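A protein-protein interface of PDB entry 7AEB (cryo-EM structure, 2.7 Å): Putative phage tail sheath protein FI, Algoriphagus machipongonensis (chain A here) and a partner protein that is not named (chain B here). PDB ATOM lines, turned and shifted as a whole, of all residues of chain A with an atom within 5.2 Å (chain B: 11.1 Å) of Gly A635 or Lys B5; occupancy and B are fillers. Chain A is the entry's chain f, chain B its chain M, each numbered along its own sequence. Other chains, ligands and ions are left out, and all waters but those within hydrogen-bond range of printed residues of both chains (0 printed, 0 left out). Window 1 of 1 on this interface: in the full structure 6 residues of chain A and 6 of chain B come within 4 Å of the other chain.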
ATOM      1  N   TRP A 523      15.928  21.765   5.953  1.00  0.00           N
ATOM      2  CA  TRP A 523      14.581  22.085   5.515  1.00  0.00           C
ATOM      3  C   TRP A 523      13.538  21.979   6.626  1.00  0.00           C
ATOM      4  O   TRP A 523      12.357  22.232   6.384  1.00  0.00           O
ATOM      5  CB  TRP A 523      14.194  21.192   4.343  1.00  0.00           C
ATOM      6  CG  TRP A 523      14.394  19.746   4.595  1.00  0.00           C
ATOM      7  CD1 TRP A 523      13.515  18.880   5.136  1.00  0.00           C
ATOM      8  CD2 TRP A 523      15.557  19.002   4.309  1.00  0.00           C
ATOM      9  NE1 TRP A 523      14.057  17.644   5.202  1.00  0.00           N
ATOM     10  CE2 TRP A 523      15.314  17.696   4.701  1.00  0.00           C
ATOM     11  CE3 TRP A 523      16.787  19.320   3.754  1.00  0.00           C
ATOM     12  CZ2 TRP A 523      16.240  16.710   4.557  1.00  0.00           C
ATOM     13  CZ3 TRP A 523      17.719  18.340   3.608  1.00  0.00           C
ATOM     14  CH2 TRP A 523      17.449  17.053   4.003  1.00  0.00           C
ATOM     15  N   GLN A 631      18.174  14.853  -3.011  1.00  0.00           N
ATOM     16  CA  GLN A 631      17.454  15.762  -2.122  1.00  0.00           C
ATOM     17  C   GLN A 631      15.973  15.433  -2.084  1.00  0.00           C
ATOM     18  O   GLN A 631      15.325  15.541  -1.036  1.00  0.00           O
ATOM     19  CB  GLN A 631      17.659  17.208  -2.563  1.00  0.00           C
ATOM     20  CG  GLN A 631      19.062  17.690  -2.382  1.00  0.00           C
ATOM     21  CD  GLN A 631      19.447  17.690  -0.951  1.00  0.00           C
ATOM     22  OE1 GLN A 631      18.744  18.253  -0.118  1.00  0.00           O
ATOM     23  NE2 GLN A 631      20.544  17.042  -0.634  1.00  0.00           N
ATOM     24  N   TRP A 632      15.439  15.008  -3.223  1.00  0.00           N
ATOM     25  CA  TRP A 632      14.049  14.602  -3.301  1.00  0.00           C
ATOM     26  C   TRP A 632      13.790  13.364  -2.447  1.00  0.00           C
ATOM     27  O   TRP A 632      12.866  13.355  -1.634  1.00  0.00           O
ATOM     28  CB  TRP A 632      13.662  14.406  -4.760  1.00  0.00           C
ATOM     29  CG  TRP A 632      12.320  13.869  -4.985  1.00  0.00           C
ATOM     30  CD1 TRP A 632      11.136  14.503  -4.820  1.00  0.00           C
ATOM     31  CD2 TRP A 632      12.008  12.590  -5.496  1.00  0.00           C
ATOM     32  NE1 TRP A 632      10.119  13.686  -5.165  1.00  0.00           N
ATOM     33  CE2 TRP A 632      10.635  12.508  -5.592  1.00  0.00           C
ATOM     34  CE3 TRP A 632      12.769  11.504  -5.885  1.00  0.00           C
ATOM     35  CZ2 TRP A 632      10.006  11.400  -6.046  1.00  0.00           C
ATOM     36  CZ3 TRP A 632      12.135  10.392  -6.352  1.00  0.00           C
ATOM     37  CH2 TRP A 632      10.783  10.343  -6.425  1.00  0.00           C
ATOM     38  N   ARG A 633      14.639  12.340  -2.554  1.00  0.00           N
ATOM     39  CA  ARG A 633      14.447  11.130  -1.758  1.00  0.00           C
ATOM     40  C   ARG A 633      14.554  11.419  -0.265  1.00  0.00           C
ATOM     41  O   ARG A 633      13.853  10.810   0.547  1.00  0.00           O
ATOM     42  CB  ARG A 633      15.477  10.070  -2.122  1.00  0.00           C
ATOM     43  CG  ARG A 633      15.424   9.532  -3.545  1.00  0.00           C
ATOM     44  CD  ARG A 633      14.222   8.725  -3.868  1.00  0.00           C
ATOM     45  NE  ARG A 633      14.197   7.451  -3.171  1.00  0.00           N
ATOM     46  CZ  ARG A 633      13.190   6.570  -3.235  1.00  0.00           C
ATOM     47  NH1 ARG A 633      12.119   6.819  -3.962  1.00  0.00           N
ATOM     48  NH2 ARG A 633      13.269   5.434  -2.565  1.00  0.00           N
ATOM     49  N   ALA A 634      15.409  12.372   0.098  1.00  0.00           N
ATOM     50  CA  ALA A 634      15.638  12.802   1.474  1.00  0.00           C
ATOM     51  C   ALA A 634      14.455  13.536   2.095  1.00  0.00           C
ATOM     52  O   ALA A 634      14.452  13.751   3.308  1.00  0.00           O
ATOM     53  CB  ALA A 634      16.852  13.714   1.539  1.00  0.00           C
ATOM     54  N   GLY A 635      13.485  13.981   1.295  1.00  0.00           N
ATOM     55  CA  GLY A 635      12.348  14.715   1.813  1.00  0.00           C
ATOM     56  C   GLY A 635      12.433  16.237   1.753  1.00  0.00           C
ATOM     57  O   GLY A 635      11.644  16.910   2.413  1.00  0.00           O
ATOM     58  N   ALA A 636      13.375  16.809   1.005  1.00  0.00           N
ATOM     59  CA  ALA A 636      13.447  18.266   0.933  1.00  0.00           C
ATOM     60  C   ALA A 636      12.509  18.833  -0.125  1.00  0.00           C
ATOM     61  O   ALA A 636      11.927  19.913   0.048  1.00  0.00           O
ATOM     62  CB  ALA A 636      14.863  18.690   0.630  1.00  0.00           C
ATOM     63  N   LEU A 637      12.388  18.121  -1.236  1.00  0.00           N
ATOM     64  CA  LEU A 637      11.612  18.577  -2.374  1.00  0.00           C
ATOM     65  C   LEU A 637      10.261  17.890  -2.413  1.00  0.00           C
ATOM     66  O   LEU A 637      10.105  16.743  -2.005  1.00  0.00           O
ATOM     67  CB  LEU A 637      12.356  18.339  -3.695  1.00  0.00           C
ATOM     68  CG  LEU A 637      13.757  18.994  -3.874  1.00  0.00           C
ATOM     69  CD1 LEU A 637      14.345  18.575  -5.218  1.00  0.00           C
ATOM     70  CD2 LEU A 637      13.659  20.514  -3.796  1.00  0.00           C
ATOM     71  N   VAL A 675       9.058  21.783   0.104  1.00  0.00           N
ATOM     72  CA  VAL A 675       8.153  21.474   1.203  1.00  0.00           C
ATOM     73  C   VAL A 675       8.026  22.640   2.184  1.00  0.00           C
ATOM     74  O   VAL A 675       9.029  23.220   2.601  1.00  0.00           O
ATOM     75  CB  VAL A 675       8.655  20.213   1.915  1.00  0.00           C
ATOM     76  CG1 VAL A 675       7.817  19.904   3.141  1.00  0.00           C
ATOM     77  CG2 VAL A 675       8.628  19.051   0.920  1.00  0.00           C
ATOM     78  N   SER B   2       5.954  15.308  -0.093  1.00  0.00           N
ATOM     79  CA  SER B   2       6.802  14.429   0.698  1.00  0.00           C
ATOM     80  C   SER B   2       6.405  12.971   0.517  1.00  0.00           C
ATOM     81  O   SER B   2       6.704  12.132   1.361  1.00  0.00           O
ATOM     82  CB  SER B   2       6.738  14.810   2.176  1.00  0.00           C
ATOM     83  OG  SER B   2       7.221  13.761   2.996  1.00  0.00           O
ATOM     84  N   GLU B   3       5.691  12.707  -0.575  1.00  0.00           N
ATOM     85  CA  GLU B   3       5.393  11.347  -0.994  1.00  0.00           C
ATOM     86  C   GLU B   3       6.661  10.637  -1.429  1.00  0.00           C
ATOM     87  O   GLU B   3       6.852   9.445  -1.157  1.00  0.00           O
ATOM     88  CB  GLU B   3       4.391  11.356  -2.149  1.00  0.00           C
ATOM     89  CG  GLU B   3       3.938   9.977  -2.587  1.00  0.00           C
ATOM     90  CD  GLU B   3       2.909  10.013  -3.699  1.00  0.00           C
ATOM     91  OE1 GLU B   3       2.598   8.946  -4.266  1.00  0.00           O
ATOM     92  OE2 GLU B   3       2.479  11.127  -4.067  1.00  0.00           O
ATOM     93  N   GLY B   4       7.539  11.373  -2.109  1.00  0.00           N
ATOM     94  CA  GLY B   4       8.762  10.850  -2.671  1.00  0.00           C
ATOM     95  C   GLY B   4       9.846  10.543  -1.674  1.00  0.00           C
ATOM     96  O   GLY B   4      10.889  10.010  -2.060  1.00  0.00           O
ATOM     97  N   LYS B   5       9.632  10.864  -0.405  1.00  0.00           N
ATOM     98  CA  LYS B   5      10.605  10.585   0.638  1.00  0.00           C
ATOM     99  C   LYS B   5      10.524   9.132   1.083  1.00  0.00           C
ATOM    100  O   LYS B   5       9.442   8.630   1.389  1.00  0.00           O
ATOM    101  CB  LYS B   5      10.367  11.502   1.833  1.00  0.00           C
ATOM    102  CG  LYS B   5      11.301  11.241   2.989  1.00  0.00           C
ATOM    103  CD  LYS B   5      10.795  11.846   4.270  1.00  0.00           C
ATOM    104  CE  LYS B   5      11.681  11.446   5.428  1.00  0.00           C
ATOM    105  NZ  LYS B   5      11.277  12.119   6.689  1.00  0.00           N
ATOM    106  N   LEU B   6      11.676   8.468   1.132  1.00  0.00           N
ATOM    107  CA  LEU B   6      11.796   7.131   1.705  1.00  0.00           C
ATOM    108  C   LEU B   6      11.838   7.250   3.224  1.00  0.00           C
ATOM    109  O   LEU B   6      12.834   7.698   3.793  1.00  0.00           O
ATOM    110  CB  LEU B   6      13.041   6.426   1.175  1.00  0.00           C
ATOM    111  CG  LEU B   6      13.258   4.971   1.611  1.00  0.00           C
ATOM    112  CD1 LEU B   6      12.175   4.071   1.069  1.00  0.00           C
ATOM    113  CD2 LEU B   6      14.613   4.469   1.175  1.00  0.00           C
ATOM    114  N   GLU B   7      10.761   6.839   3.884  1.00  0.00           N
ATOM    115  CA  GLU B   7      10.693   6.901   5.337  1.00  0.00           C
ATOM    116  C   GLU B   7      11.467   5.745   5.964  1.00  0.00           C
ATOM    117  O   GLU B   7      11.508   4.636   5.427  1.00  0.00           O
ATOM    118  CB  GLU B   7       9.230   6.876   5.789  1.00  0.00           C
ATOM    119  CG  GLU B   7       9.002   7.199   7.261  1.00  0.00           C
ATOM    120  CD  GLU B   7       9.076   8.688   7.572  1.00  0.00           C
ATOM    121  OE1 GLU B   7       9.222   9.040   8.756  1.00  0.00           O
ATOM    122  OE2 GLU B   7       8.981   9.510   6.638  1.00  0.00           O
ATOM    123  N   LYS B   8      12.092   6.016   7.108  1.00  0.00           N
ATOM    124  CA  LYS B   8      12.898   5.048   7.836  1.00  0.00           C
ATOM    125  C   LYS B   8      12.233   4.698   9.160  1.00  0.00           C
ATOM    126  O   LYS B   8      11.582   5.541   9.781  1.00  0.00           O
ATOM    127  CB  LYS B   8      14.300   5.602   8.076  1.00  0.00           C
ATOM    128  CG  LYS B   8      15.148   5.648   6.829  1.00  0.00           C
ATOM    129  CD  LYS B   8      15.610   4.262   6.447  1.00  0.00           C
ATOM    130  CE  LYS B   8      16.028   4.204   5.003  1.00  0.00           C
ATOM    131  NZ  LYS B   8      17.058   5.217   4.692  1.00  0.00           N
ATOM    132  N   LEU B   9      12.404   3.450   9.590  1.00  0.00           N
ATOM    133  CA  LEU B   9      11.745   2.944  10.790  1.00  0.00           C
ATOM    134  C   LEU B   9      12.388   3.525  12.050  1.00  0.00           C
ATOM    135  O   LEU B   9      13.600   3.726  12.108  1.00  0.00           O
ATOM    136  CB  LEU B   9      11.802   1.413  10.777  1.00  0.00           C
ATOM    137  CG  LEU B   9      11.562   0.488  11.975  1.00  0.00           C
ATOM    138  CD1 LEU B   9      10.247   0.741  12.615  1.00  0.00           C
ATOM    139  CD2 LEU B   9      11.599  -0.937  11.526  1.00  0.00           C
ATOM    140  N   ARG B  10      11.557   3.867  13.035  1.00  0.00           N
ATOM    141  CA  ARG B  10      11.987   4.449  14.300  1.00  0.00           C
ATOM    142  C   ARG B  10      11.483   3.682  15.504  1.00  0.00           C
ATOM    143  O   ARG B  10      10.408   3.127  15.480  1.00  0.00           O
ATOM    144  CB  ARG B  10      11.440   5.845  14.467  1.00  0.00           C
ATOM    145  CG  ARG B  10      12.067   6.896  13.612  1.00  0.00           C
ATOM    146  CD  ARG B  10      11.936   8.266  14.246  1.00  0.00           C
ATOM    147  NE  ARG B  10      10.641   8.468  14.878  1.00  0.00           N
ATOM    148  CZ  ARG B  10      10.396   9.388  15.802  1.00  0.00           C
ATOM    149  NH1 ARG B  10      11.355  10.184  16.213  1.00  0.00           N
ATOM    150  NH2 ARG B  10       9.197   9.497  16.331  1.00  0.00           N
ATOM    151  N   GLU B  27      15.866   7.439  21.496  1.00  0.00           N
ATOM    152  CA  GLU B  27      15.251   7.259  20.190  1.00  0.00           C
ATOM    153  C   GLU B  27      16.264   6.664  19.222  1.00  0.00           C
ATOM    154  O   GLU B  27      17.371   7.188  19.078  1.00  0.00           O
ATOM    155  CB  GLU B  27      14.708   8.588  19.660  1.00  0.00           C
ATOM    156  CG  GLU B  27      14.486   8.626  18.172  1.00  0.00           C
ATOM    157  CD  GLU B  27      13.948   9.951  17.707  1.00  0.00           C
ATOM    158  OE1 GLU B  27      12.898  10.390  18.227  1.00  0.00           O
ATOM    159  OE2 GLU B  27      14.561  10.567  16.814  1.00  0.00           O
ATOM    160  N   ILE B  29      16.903   5.370  15.213  1.00  0.00           N
ATOM    161  CA  ILE B  29      16.484   5.437  13.819  1.00  0.00           C
ATOM    162  C   ILE B  29      17.398   4.523  13.018  1.00  0.00           C
ATOM    163  O   ILE B  29      18.623   4.627  13.120  1.00  0.00           O
ATOM    164  CB  ILE B  29      16.530   6.874  13.264  1.00  0.00           C
ATOM    165  CG1 ILE B  29      15.743   7.832  14.155  1.00  0.00           C
ATOM    166  CG2 ILE B  29      15.971   6.929  11.859  1.00  0.00           C
ATOM    167  CD1 ILE B  29      16.064   9.274  13.932  1.00  0.00           C
ATOM    168  N   THR B  30      16.810   3.637  12.224  1.00  0.00           N
ATOM    169  CA  THR B  30      17.597   2.709  11.431  1.00  0.00           C
ATOM    170  C   THR B  30      18.150   3.396  10.181  1.00  0.00           C
ATOM    171  O   THR B  30      17.698   4.466   9.767  1.00  0.00           O
ATOM    172  CB  THR B  30      16.762   1.482  11.057  1.00  0.00           C
ATOM    173  OG1 THR B  30      17.627   0.409  10.673  1.00  0.00           O
ATOM    174  CG2 THR B  30      15.821   1.778   9.905  1.00  0.00           C
ATOM    175  N   ASN B  33      15.949  -0.218   6.148  1.00  0.00           N
ATOM    176  CA  ASN B  33      14.646  -0.758   6.497  1.00  0.00           C
ATOM    177  C   ASN B  33      14.648  -2.281   6.397  1.00  0.00           C
ATOM    178  O   ASN B  33      15.375  -2.853   5.582  1.00  0.00           O
ATOM    179  CB  ASN B  33      13.580  -0.197   5.556  1.00  0.00           C
ATOM    180  CG  ASN B  33      13.032   1.128   6.019  1.00  0.00           C
ATOM    181  OD1 ASN B  33      12.767   1.311   7.194  1.00  0.00           O
ATOM    182  ND2 ASN B  33      12.864   2.057   5.096  1.00  0.00           N
ATOM    183  N   TYR B  83      25.584   7.988   3.218  1.00  0.00           N
ATOM    184  CA  TYR B  83      26.197   7.785   4.519  1.00  0.00           C
ATOM    185  C   TYR B  83      27.712   7.828   4.402  1.00  0.00           C
ATOM    186  O   TYR B  83      28.274   7.693   3.314  1.00  0.00           O
ATOM    187  CB  TYR B  83      25.755   6.458   5.134  1.00  0.00           C
ATOM    188  CG  TYR B  83      24.266   6.377   5.299  1.00  0.00           C
ATOM    189  CD1 TYR B  83      23.562   7.431   5.855  1.00  0.00           C
ATOM    190  CD2 TYR B  83      23.557   5.259   4.880  1.00  0.00           C
ATOM    191  CE1 TYR B  83      22.190   7.381   6.001  1.00  0.00           C
ATOM    192  CE2 TYR B  83      22.181   5.193   5.024  1.00  0.00           C
ATOM    193  CZ  TYR B  83      21.502   6.259   5.587  1.00  0.00           C
ATOM    194  OH  TYR B  83      20.137   6.213   5.740  1.00  0.00           O
ATOM    195  N   THR B 117       7.260   2.660  15.038  1.00  0.00           N
ATOM    196  CA  THR B 117       6.494   3.348  14.006  1.00  0.00           C
ATOM    197  C   THR B 117       7.226   3.327  12.673  1.00  0.00           C
ATOM    198  O   THR B 117       8.396   3.711  12.596  1.00  0.00           O
ATOM    199  CB  THR B 117       6.192   4.810  14.379  1.00  0.00           C
ATOM    200  OG1 THR B 117       7.385   5.461  14.831  1.00  0.00           O
ATOM    201  CG2 THR B 117       5.131   4.900  15.454  1.00  0.00           C
ATOM    202  N   TRP B 118       6.528   2.901  11.626  1.00  0.00           N
ATOM    203  CA  TRP B 118       7.035   2.997  10.259  1.00  0.00           C
ATOM    204  C   TRP B 118       5.845   3.025   9.314  1.00  0.00           C
ATOM    205  O   TRP B 118       5.212   1.991   9.096  1.00  0.00           O
ATOM    206  CB  TRP B 118       7.956   1.831   9.924  1.00  0.00           C
ATOM    207  CG  TRP B 118       8.447   1.816   8.506  1.00  0.00           C
ATOM    208  CD1 TRP B 118       8.776   2.890   7.742  1.00  0.00           C
ATOM    209  CD2 TRP B 118       8.675   0.663   7.694  1.00  0.00           C
ATOM    210  NE1 TRP B 118       9.178   2.483   6.501  1.00  0.00           N
ATOM    211  CE2 TRP B 118       9.129   1.119   6.445  1.00  0.00           C
ATOM    212  CE3 TRP B 118       8.535  -0.712   7.899  1.00  0.00           C
ATOM    213  CZ2 TRP B 118       9.441   0.251   5.403  1.00  0.00           C
ATOM    214  CZ3 TRP B 118       8.851  -1.571   6.866  1.00  0.00           C
ATOM    215  CH2 TRP B 118       9.300  -1.086   5.633  1.00  0.00           C
ATOM    216  N   GLY B 119       5.560   4.189   8.741  1.00  0.00           N
ATOM    217  CA  GLY B 119       4.458   4.314   7.804  1.00  0.00           C
ATOM    218  C   GLY B 119       3.115   4.135   8.477  1.00  0.00           C
ATOM    219  O   GLY B 119       2.720   4.915   9.343  1.00  0.00           O
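NZ of Lys B5 lies within salt-bridge range of OE2 of Glu B7 (3.5 Å).
Of chain B, only Gly B4 comes within 4 Å of Trp A632.
Arg A633 touches just these residues of chain B: Gly B4 (3.7 Å), Lys B5 (3.3 Å) and Leu B6 (3.3 Å).
Of chain B, only Lys B5 comes within 4 Å of Gly A635.
Printed residues of chain A within 4 Å of Gly B4: Trp A632 (3.6 Å) and Arg A633 (3.7 Å).
Of the printed residues of chain A, Lys B5 touches Arg A633 and Gly A635.
Of the printed residues of chain A, Leu B6 touches Arg A633 (3.3 Å).
The nearest printed residue of chain A that does not touch Leu B6 is Ala A634 (5.5 Å).
The backbone NH of Leu B6 lies within hydrogen-bond range of the backbone carbonyl oxygen of Arg A633 (3.3 Å).
Among the printed residues, merely in contact across the chains: Arg A633 with Lys B5, Trp A632 with Gly B4, Arg A633 with Gly B4 and Gly A635 with Lys B5.
Of the 9 printed residues of chain A, 3 touch a printed residue of chain B.
Printed residues of chain A that touch a printed residue of chain B: Trp A632, Arg A633 and Gly A635.
Of the 17 printed residues of chain B, 3 touch a printed residue of chain A.
Printed residues of chain B that touch a printed residue of chain A: Gly B4, Lys B5 and Leu B6.
Hydrophobic or aromatic side chains of chain B within 4 Å of the printed part of chain A: Leu B6.
Along chain B the printed residues that touch a printed residue of chain A span positions 4 to 6.
Among the printed residues, 5 pairs touch across the chains.
Among the printed residues, no Asp or Glu carboxylate lies within 4 Å of a Lys or Arg side-chain nitrogen of the other chain.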
